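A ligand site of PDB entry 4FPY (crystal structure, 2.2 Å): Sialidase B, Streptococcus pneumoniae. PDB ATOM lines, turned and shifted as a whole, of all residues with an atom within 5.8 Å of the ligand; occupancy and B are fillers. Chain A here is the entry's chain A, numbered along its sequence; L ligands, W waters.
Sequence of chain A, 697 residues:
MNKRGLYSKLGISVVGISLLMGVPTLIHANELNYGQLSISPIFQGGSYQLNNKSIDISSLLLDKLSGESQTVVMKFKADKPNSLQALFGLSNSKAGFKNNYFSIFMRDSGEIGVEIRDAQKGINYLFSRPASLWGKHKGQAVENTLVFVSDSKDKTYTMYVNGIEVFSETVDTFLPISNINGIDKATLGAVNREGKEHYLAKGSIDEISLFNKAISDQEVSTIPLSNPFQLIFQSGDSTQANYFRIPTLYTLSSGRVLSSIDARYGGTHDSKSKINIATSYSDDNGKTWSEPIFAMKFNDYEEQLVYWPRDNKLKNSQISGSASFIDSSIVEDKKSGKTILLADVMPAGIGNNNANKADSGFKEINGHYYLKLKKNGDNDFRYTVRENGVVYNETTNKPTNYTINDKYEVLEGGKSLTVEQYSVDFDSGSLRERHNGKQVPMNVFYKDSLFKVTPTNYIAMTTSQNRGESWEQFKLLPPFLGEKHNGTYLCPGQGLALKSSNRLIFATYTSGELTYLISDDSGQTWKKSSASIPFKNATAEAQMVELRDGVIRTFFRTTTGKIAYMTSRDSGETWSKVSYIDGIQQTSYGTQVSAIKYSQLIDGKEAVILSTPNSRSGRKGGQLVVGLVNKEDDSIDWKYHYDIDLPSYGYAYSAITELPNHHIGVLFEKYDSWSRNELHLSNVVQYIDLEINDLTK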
ATOM      1  N   ARG A 245     -14.213  32.422   8.526  1.00  0.00           N
ATOM      2  CA  ARG A 245     -15.472  31.885   8.026  1.00  0.00           C
ATOM      3  C   ARG A 245     -16.596  32.254   8.999  1.00  0.00           C
ATOM      4  O   ARG A 245     -16.337  32.659  10.133  1.00  0.00           O
ATOM      5  CB  ARG A 245     -15.419  30.359   7.871  1.00  0.00           C
ATOM      6  CG  ARG A 245     -14.801  29.832   6.554  1.00  0.00           C
ATOM      7  CD  ARG A 245     -15.460  28.469   6.121  1.00  0.00           C
ATOM      8  NE  ARG A 245     -16.905  28.608   5.915  1.00  0.00           N
ATOM      9  CZ  ARG A 245     -17.745  27.597   5.690  1.00  0.00           C
ATOM     10  NH1 ARG A 245     -17.299  26.333   5.626  1.00  0.00           N
ATOM     11  NH2 ARG A 245     -19.040  27.839   5.529  1.00  0.00           N
ATOM     12  N   ILE A 246     -17.828  32.059   8.546  1.00  0.00           N
ATOM     13  CA  ILE A 246     -18.998  32.245   9.390  1.00  0.00           C
ATOM     14  C   ILE A 246     -19.111  33.668   9.930  1.00  0.00           C
ATOM     15  O   ILE A 246     -19.043  33.883  11.135  1.00  0.00           O
ATOM     16  CB  ILE A 246     -19.023  31.248  10.566  1.00  0.00           C
ATOM     17  CG1 ILE A 246     -18.406  29.886  10.171  1.00  0.00           C
ATOM     18  CG2 ILE A 246     -20.423  31.067  11.053  1.00  0.00           C
ATOM     19  CD1 ILE A 246     -19.164  29.144   9.036  1.00  0.00           C
ATOM     20  N   ARG A 264     -10.128  31.202  11.892  1.00  0.00           N
ATOM     21  CA  ARG A 264      -9.750  29.804  11.685  1.00  0.00           C
ATOM     22  C   ARG A 264      -8.273  29.658  11.360  1.00  0.00           C
ATOM     23  O   ARG A 264      -7.781  30.229  10.381  1.00  0.00           O
ATOM     24  CB  ARG A 264     -10.637  29.151  10.615  1.00  0.00           C
ATOM     25  CG  ARG A 264     -12.144  29.230  10.917  1.00  0.00           C
ATOM     26  CD  ARG A 264     -12.960  28.298  10.023  1.00  0.00           C
ATOM     27  NE  ARG A 264     -14.308  28.088  10.526  1.00  0.00           N
ATOM     28  CZ  ARG A 264     -15.161  27.170  10.053  1.00  0.00           C
ATOM     29  NH1 ARG A 264     -14.801  26.366   9.063  1.00  0.00           N
ATOM     30  NH2 ARG A 264     -16.371  27.070  10.561  1.00  0.00           N
ATOM     31  N   ASP A 270     -13.817  23.146   9.195  1.00  0.00           N
ATOM     32  CA  ASP A 270     -14.620  23.147  10.428  1.00  0.00           C
ATOM     33  C   ASP A 270     -13.822  22.331  11.453  1.00  0.00           C
ATOM     34  O   ASP A 270     -13.007  21.507  11.047  1.00  0.00           O
ATOM     35  CB  ASP A 270     -15.957  22.427  10.199  1.00  0.00           C
ATOM     36  CG  ASP A 270     -16.966  23.232   9.380  1.00  0.00           C
ATOM     37  OD1 ASP A 270     -18.065  22.699   9.162  1.00  0.00           O
ATOM     38  OD2 ASP A 270     -16.700  24.391   8.980  1.00  0.00           O
ATOM     39  N   SER A 271     -14.034  22.535  12.744  1.00  0.00           N
ATOM     40  CA  SER A 271     -13.479  21.606  13.744  1.00  0.00           C
ATOM     41  C   SER A 271     -13.516  20.144  13.212  1.00  0.00           C
ATOM     42  O   SER A 271     -14.541  19.732  12.685  1.00  0.00           O
ATOM     43  CB  SER A 271     -14.290  21.695  15.048  1.00  0.00           C
ATOM     44  OG  SER A 271     -14.362  23.033  15.535  1.00  0.00           O
ATOM     45  N   LYS A 272     -12.436  19.375  13.361  1.00  0.00           N
ATOM     46  CA  LYS A 272     -11.290  19.705  14.208  1.00  0.00           C
ATOM     47  C   LYS A 272     -10.229  20.616  13.586  1.00  0.00           C
ATOM     48  O   LYS A 272      -9.742  20.405  12.464  1.00  0.00           O
ATOM     49  CB  LYS A 272     -10.627  18.427  14.728  1.00  0.00           C
ATOM     50  CG  LYS A 272     -10.223  17.439  13.663  1.00  0.00           C
ATOM     51  CD  LYS A 272      -9.987  16.066  14.280  1.00  0.00           C
ATOM     52  CE  LYS A 272      -9.578  15.032  13.243  1.00  0.00           C
ATOM     53  NZ  LYS A 272      -8.149  15.153  12.839  1.00  0.00           N
ATOM     54  N   ILE A 326     -16.791  27.320  17.238  1.00  0.00           N
ATOM     55  CA  ILE A 326     -17.243  27.350  15.851  1.00  0.00           C
ATOM     56  C   ILE A 326     -18.673  27.890  15.828  1.00  0.00           C
ATOM     57  O   ILE A 326     -19.433  27.615  16.751  1.00  0.00           O
ATOM     58  CB  ILE A 326     -17.121  25.948  15.171  1.00  0.00           C
ATOM     59  CG1 ILE A 326     -17.610  25.992  13.726  1.00  0.00           C
ATOM     60  CG2 ILE A 326     -17.851  24.858  15.976  1.00  0.00           C
ATOM     61  CD1 ILE A 326     -17.116  24.802  12.909  1.00  0.00           C
ATOM     62  N   ASP A 327     -19.019  28.692  14.821  1.00  0.00           N
ATOM     63  CA  ASP A 327     -20.380  29.227  14.644  1.00  0.00           C
ATOM     64  C   ASP A 327     -20.827  30.188  15.766  1.00  0.00           C
ATOM     65  O   ASP A 327     -21.373  29.745  16.775  1.00  0.00           O
ATOM     66  CB  ASP A 327     -21.417  28.093  14.513  1.00  0.00           C
ATOM     67  CG  ASP A 327     -21.292  27.322  13.207  1.00  0.00           C
ATOM     68  OD1 ASP A 327     -20.489  27.725  12.339  1.00  0.00           O
ATOM     69  OD2 ASP A 327     -22.018  26.301  13.054  1.00  0.00           O
ATOM     70  N   ASP A 344     -20.708  27.568  19.380  1.00  0.00           N
ATOM     71  CA  ASP A 344     -20.461  26.164  19.729  1.00  0.00           C
ATOM     72  C   ASP A 344     -19.074  26.044  20.322  1.00  0.00           C
ATOM     73  O   ASP A 344     -18.158  26.775  19.940  1.00  0.00           O
ATOM     74  CB  ASP A 344     -20.541  25.240  18.510  1.00  0.00           C
ATOM     75  CG  ASP A 344     -21.867  25.326  17.780  1.00  0.00           C
ATOM     76  OD1 ASP A 344     -22.921  25.470  18.434  1.00  0.00           O
ATOM     77  OD2 ASP A 344     -21.851  25.241  16.537  1.00  0.00           O
ATOM     78  N   MET A 346     -16.006  23.108  21.242  1.00  0.00           N
ATOM     79  CA  MET A 346     -15.532  21.748  21.076  1.00  0.00           C
ATOM     80  C   MET A 346     -14.208  21.505  21.788  1.00  0.00           C
ATOM     81  O   MET A 346     -13.242  22.235  21.577  1.00  0.00           O
ATOM     82  CB  MET A 346     -15.451  21.411  19.595  1.00  0.00           C
ATOM     83  CG  MET A 346     -16.843  21.202  18.999  1.00  0.00           C
ATOM     84  SD  MET A 346     -16.896  20.922  17.247  1.00  0.00           S
ATOM     85  CE  MET A 346     -18.500  20.148  17.127  1.00  0.00           C
ATOM     86  N   TYR A 489     -26.959  22.575  17.861  1.00  0.00           N
ATOM     87  CA  TYR A 489     -25.957  23.368  17.160  1.00  0.00           C
ATOM     88  C   TYR A 489     -26.454  24.794  16.943  1.00  0.00           C
ATOM     89  O   TYR A 489     -27.520  25.007  16.377  1.00  0.00           O
ATOM     90  CB  TYR A 489     -25.626  22.707  15.814  1.00  0.00           C
ATOM     91  CG  TYR A 489     -24.847  21.421  15.951  1.00  0.00           C
ATOM     92  CD1 TYR A 489     -23.473  21.448  16.153  1.00  0.00           C
ATOM     93  CD2 TYR A 489     -25.485  20.175  15.882  1.00  0.00           C
ATOM     94  CE1 TYR A 489     -22.756  20.285  16.284  1.00  0.00           C
ATOM     95  CE2 TYR A 489     -24.767  19.003  16.009  1.00  0.00           C
ATOM     96  CZ  TYR A 489     -23.400  19.070  16.221  1.00  0.00           C
ATOM     97  OH  TYR A 489     -22.660  17.926  16.358  1.00  0.00           O
ATOM     98  N   TYR A 509     -30.156  24.124  16.053  1.00  0.00           N
ATOM     99  CA  TYR A 509     -30.731  22.966  15.370  1.00  0.00           C
ATOM    100  C   TYR A 509     -30.158  21.647  15.856  1.00  0.00           C
ATOM    101  O   TYR A 509     -29.060  21.568  16.396  1.00  0.00           O
ATOM    102  CB  TYR A 509     -30.533  23.067  13.850  1.00  0.00           C
ATOM    103  CG  TYR A 509     -29.096  23.021  13.378  1.00  0.00           C
ATOM    104  CD1 TYR A 509     -28.495  21.821  13.015  1.00  0.00           C
ATOM    105  CD2 TYR A 509     -28.342  24.182  13.276  1.00  0.00           C
ATOM    106  CE1 TYR A 509     -27.173  21.772  12.569  1.00  0.00           C
ATOM    107  CE2 TYR A 509     -27.034  24.153  12.835  1.00  0.00           C
ATOM    108  CZ  TYR A 509     -26.444  22.945  12.490  1.00  0.00           C
ATOM    109  OH  TYR A 509     -25.136  22.906  12.045  1.00  0.00           O
ATOM    110  N   THR A 539     -28.354  20.231   8.315  1.00  0.00           N
ATOM    111  CA  THR A 539     -27.696  21.383   8.873  1.00  0.00           C
ATOM    112  C   THR A 539     -28.685  22.513   8.707  1.00  0.00           C
ATOM    113  O   THR A 539     -28.623  23.250   7.738  1.00  0.00           O
ATOM    114  CB  THR A 539     -26.409  21.701   8.085  1.00  0.00           C
ATOM    115  OG1 THR A 539     -25.598  20.522   8.040  1.00  0.00           O
ATOM    116  CG2 THR A 539     -25.629  22.821   8.739  1.00  0.00           C
ATOM    117  N   GLU A 541     -29.445  25.555   9.611  1.00  0.00           N
ATOM    118  CA  GLU A 541     -29.119  26.906  10.035  1.00  0.00           C
ATOM    119  C   GLU A 541     -30.290  27.831   9.760  1.00  0.00           C
ATOM    120  O   GLU A 541     -30.741  27.968   8.616  1.00  0.00           O
ATOM    121  CB  GLU A 541     -27.829  27.385   9.331  1.00  0.00           C
ATOM    122  CG  GLU A 541     -26.628  26.505   9.723  1.00  0.00           C
ATOM    123  CD  GLU A 541     -25.542  26.448   8.670  1.00  0.00           C
ATOM    124  OE1 GLU A 541     -24.386  26.108   9.039  1.00  0.00           O
ATOM    125  OE2 GLU A 541     -25.820  26.747   7.493  1.00  0.00           O
ATOM    126  N   ARG A 557     -32.011  26.715   6.307  1.00  0.00           N
ATOM    127  CA  ARG A 557     -31.349  25.851   5.339  1.00  0.00           C
ATOM    128  C   ARG A 557     -31.900  24.428   5.442  1.00  0.00           C
ATOM    129  O   ARG A 557     -32.185  23.957   6.543  1.00  0.00           O
ATOM    130  CB  ARG A 557     -29.854  25.864   5.645  1.00  0.00           C
ATOM    131  CG  ARG A 557     -29.030  24.783   4.961  1.00  0.00           C
ATOM    132  CD  ARG A 557     -27.563  24.911   5.378  1.00  0.00           C
ATOM    133  NE  ARG A 557     -26.740  23.854   4.808  1.00  0.00           N
ATOM    134  CZ  ARG A 557     -25.422  23.804   4.937  1.00  0.00           C
ATOM    135  NH1 ARG A 557     -24.775  24.759   5.608  1.00  0.00           N
ATOM    136  NH2 ARG A 557     -24.744  22.809   4.393  1.00  0.00           N
ATOM    137  N   GLY A 590     -27.221  22.754   0.671  1.00  0.00           N
ATOM    138  CA  GLY A 590     -27.684  24.042   1.134  1.00  0.00           C
ATOM    139  C   GLY A 590     -26.611  24.955   1.699  1.00  0.00           C
ATOM    140  O   GLY A 590     -25.461  24.555   1.862  1.00  0.00           O
ATOM    141  N   ARG A 619     -22.006  27.154  -4.345  1.00  0.00           N
ATOM    142  CA  ARG A 619     -22.143  28.354  -3.538  1.00  0.00           C
ATOM    143  C   ARG A 619     -21.652  29.566  -4.330  1.00  0.00           C
ATOM    144  O   ARG A 619     -20.511  30.021  -4.202  1.00  0.00           O
ATOM    145  CB  ARG A 619     -21.425  28.182  -2.192  1.00  0.00           C
ATOM    146  CG  ARG A 619     -22.071  27.052  -1.321  1.00  0.00           C
ATOM    147  CD  ARG A 619     -21.525  27.000   0.095  1.00  0.00           C
ATOM    148  NE  ARG A 619     -22.342  26.189   1.009  1.00  0.00           N
ATOM    149  CZ  ARG A 619     -21.911  25.754   2.201  1.00  0.00           C
ATOM    150  NH1 ARG A 619     -20.671  26.054   2.593  1.00  0.00           N
ATOM    151  NH2 ARG A 619     -22.694  25.025   2.986  1.00  0.00           N
ATOM    152  N   TYR A 653     -21.680  31.598   3.036  1.00  0.00           N
ATOM    153  CA  TYR A 653     -22.309  32.111   4.263  1.00  0.00           C
ATOM    154  C   TYR A 653     -22.332  33.631   4.240  1.00  0.00           C
ATOM    155  O   TYR A 653     -21.460  34.270   3.651  1.00  0.00           O
ATOM    156  CB  TYR A 653     -21.600  31.625   5.525  1.00  0.00           C
ATOM    157  CG  TYR A 653     -21.947  30.221   5.975  1.00  0.00           C
ATOM    158  CD1 TYR A 653     -22.025  29.172   5.073  1.00  0.00           C
ATOM    159  CD2 TYR A 653     -22.159  29.947   7.322  1.00  0.00           C
ATOM    160  CE1 TYR A 653     -22.305  27.874   5.485  1.00  0.00           C
ATOM    161  CE2 TYR A 653     -22.450  28.650   7.756  1.00  0.00           C
ATOM    162  CZ  TYR A 653     -22.522  27.612   6.829  1.00  0.00           C
ATOM    163  OH  TYR A 653     -22.810  26.321   7.250  1.00  0.00           O
ATOM    164  N   SER A 673     -17.389  27.921  -0.255  1.00  0.00           N
ATOM    165  CA  SER A 673     -16.853  27.359   0.976  1.00  0.00           C
ATOM    166  C   SER A 673     -17.240  25.883   1.174  1.00  0.00           C
ATOM    167  O   SER A 673     -16.949  25.278   2.204  1.00  0.00           O
ATOM    168  CB  SER A 673     -17.278  28.212   2.189  1.00  0.00           C
ATOM    169  OG  SER A 673     -18.684  28.177   2.383  1.00  0.00           O
ATOM    170  N   TRP A 674     -17.910  25.321   0.177  1.00  0.00           N
ATOM    171  CA  TRP A 674     -18.180  23.879   0.140  1.00  0.00           C
ATOM    172  C   TRP A 674     -17.109  23.177  -0.713  1.00  0.00           C
ATOM    173  O   TRP A 674     -16.597  22.124  -0.350  1.00  0.00           O
ATOM    174  CB  TRP A 674     -19.562  23.584  -0.437  1.00  0.00           C
ATOM    175  CG  TRP A 674     -19.984  22.148  -0.301  1.00  0.00           C
ATOM    176  CD1 TRP A 674     -19.847  21.160  -1.232  1.00  0.00           C
ATOM    177  CD2 TRP A 674     -20.608  21.541   0.845  1.00  0.00           C
ATOM    178  NE1 TRP A 674     -20.346  19.965  -0.739  1.00  0.00           N
ATOM    179  CE2 TRP A 674     -20.820  20.183   0.534  1.00  0.00           C
ATOM    180  CE3 TRP A 674     -21.008  22.020   2.105  1.00  0.00           C
ATOM    181  CZ2 TRP A 674     -21.423  19.285   1.428  1.00  0.00           C
ATOM    182  CZ3 TRP A 674     -21.613  21.141   2.984  1.00  0.00           C
ATOM    183  CH2 TRP A 674     -21.805  19.784   2.646  1.00  0.00           C
HETATM  184  C1  LIG L   1     -20.540  22.879  14.519  1.00  0.00           C
HETATM  185  C2  LIG L   1     -19.466  21.981  14.471  1.00  0.00           C
HETATM  186  C3  LIG L   1     -21.241  23.170  13.344  1.00  0.00           C
HETATM  187  C4  LIG L   1     -19.790  21.673  12.102  1.00  0.00           C
HETATM  188  C5  LIG L   1     -21.138  23.456   8.520  1.00  0.00           C
HETATM  189  C6  LIG L   1     -20.414  24.392   7.545  1.00  0.00           C
HETATM  190  C7  LIG L   1     -21.575  22.836  10.841  1.00  0.00           C
HETATM  191  C8  LIG L   1     -19.090  21.392  13.281  1.00  0.00           C
HETATM  192  C9  LIG L   1     -20.868  22.538  12.150  1.00  0.00           C
HETATM  193  N1  LIG L   1     -20.711  23.604   9.927  1.00  0.00           N
HETATM  194  O1  LIG L   1     -19.907  22.599   5.746  1.00  0.00           O
HETATM  195  O2  LIG L   1     -21.951  23.895   5.426  1.00  0.00           O
HETATM  196  O3  LIG L   1     -19.791  24.874   4.981  1.00  0.00           O
HETATM  197  S1  LIG L   1     -20.515  23.922   5.844  1.00  0.00           S
HETATM  198 BR1  LIG L   1     -17.603  20.140  13.202  1.00  0.00          BR
HETATM  199  O   HOH W   1     -16.790  22.629   4.311  1.00  0.00           O
HETATM  200  O   HOH W   2     -23.835  25.011  11.472  1.00  0.00           O
HETATM  201  O   HOH W   3     -19.952  25.955  10.230  1.00  0.00           O
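NH2 of Arg 619 is in salt-bridge range of O2 of the ligand, 2.8 Å away.
N1 of the ligand is in salt-bridge range of OD1 of Asp 270 (2.9 Å).
An oxygen (O2) of the ligand is in salt-bridge range of the guanidinium group (NH1) of Arg 557 (3.0 Å).
An oxygen (O3) of the ligand is in salt-bridge range of the guanidinium group (NH1) of Arg 245, at 3.0 Å.
The side-chain hydroxyl of Tyr 653 lies close to an oxygen (O2) of the ligand, at 3.2 Å.
The guanidinium group of Arg 619 lies within hydrogen-bond range of the backbone carbonyl oxygen of Gly 590 (3.0 Å).
The side-chain carboxylate of Asp 270 is in salt-bridge range of the guanidinium group of Arg 264 (2.7 Å).
The guanidinium group of Arg 557 lies within hydrogen-bond range of the side-chain hydroxyl of Tyr 653 (3.0 Å).
OE2 of Glu 541 is in salt-bridge range of NH1 of Arg 557 (2.9 Å).
The guanidinium group (NH2) of Arg 245 sits at hydrogen-bond distance from the side-chain hydroxyl (OG) of Ser 673, 3.2 Å away.
The side-chain hydroxyl (OH) of Tyr 653 is in hydrogen-bond range of the side-chain carboxylate (OE2) of Glu 541 (3.0 Å).
OG of Ser 271 sits close to SD of Met 346 (3.7 Å).
The backbone NH of Tyr 489 is in hydrogen-bond range of the backbone carbonyl oxygen of Tyr 509 (2.8 Å).
Residues that only touch the ligand: Ser 271 (3.1 Å), Asp 327 (3.2 Å), Met 346 (3.4 Å), Asp 344 (3.4 Å), Trp 674 (3.6 Å), Ile 326 (3.6 Å), Tyr 489 (3.6 Å), Tyr 509 (3.8 Å) and Ser 673 (3.99 Å).
Hydrophobic or aromatic side chains within 4 Å of the ligand: Ile 326, Met 346, Tyr 489, Tyr 653 and Trp 674.
Of the 20 residues printed, 14 come within 4 Å of the ligand.
The nearest printed residue that does not touch the ligand is Glu 541 (4.2 Å).
Water W3 bridges N1 of the ligand (2.5 Å) and OD1 of Asp 327 (2.8 Å).
Water W2 lies within hydrogen-bond range of OH of Tyr 509, OE1 of Glu 541 and OD2 of Asp 327.
Water W1 lies within hydrogen-bond range of the backbone carbonyl oxygen (O) of Ser 673 (3.4 Å) and an oxygen (O1) of the ligand (3.4 Å).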
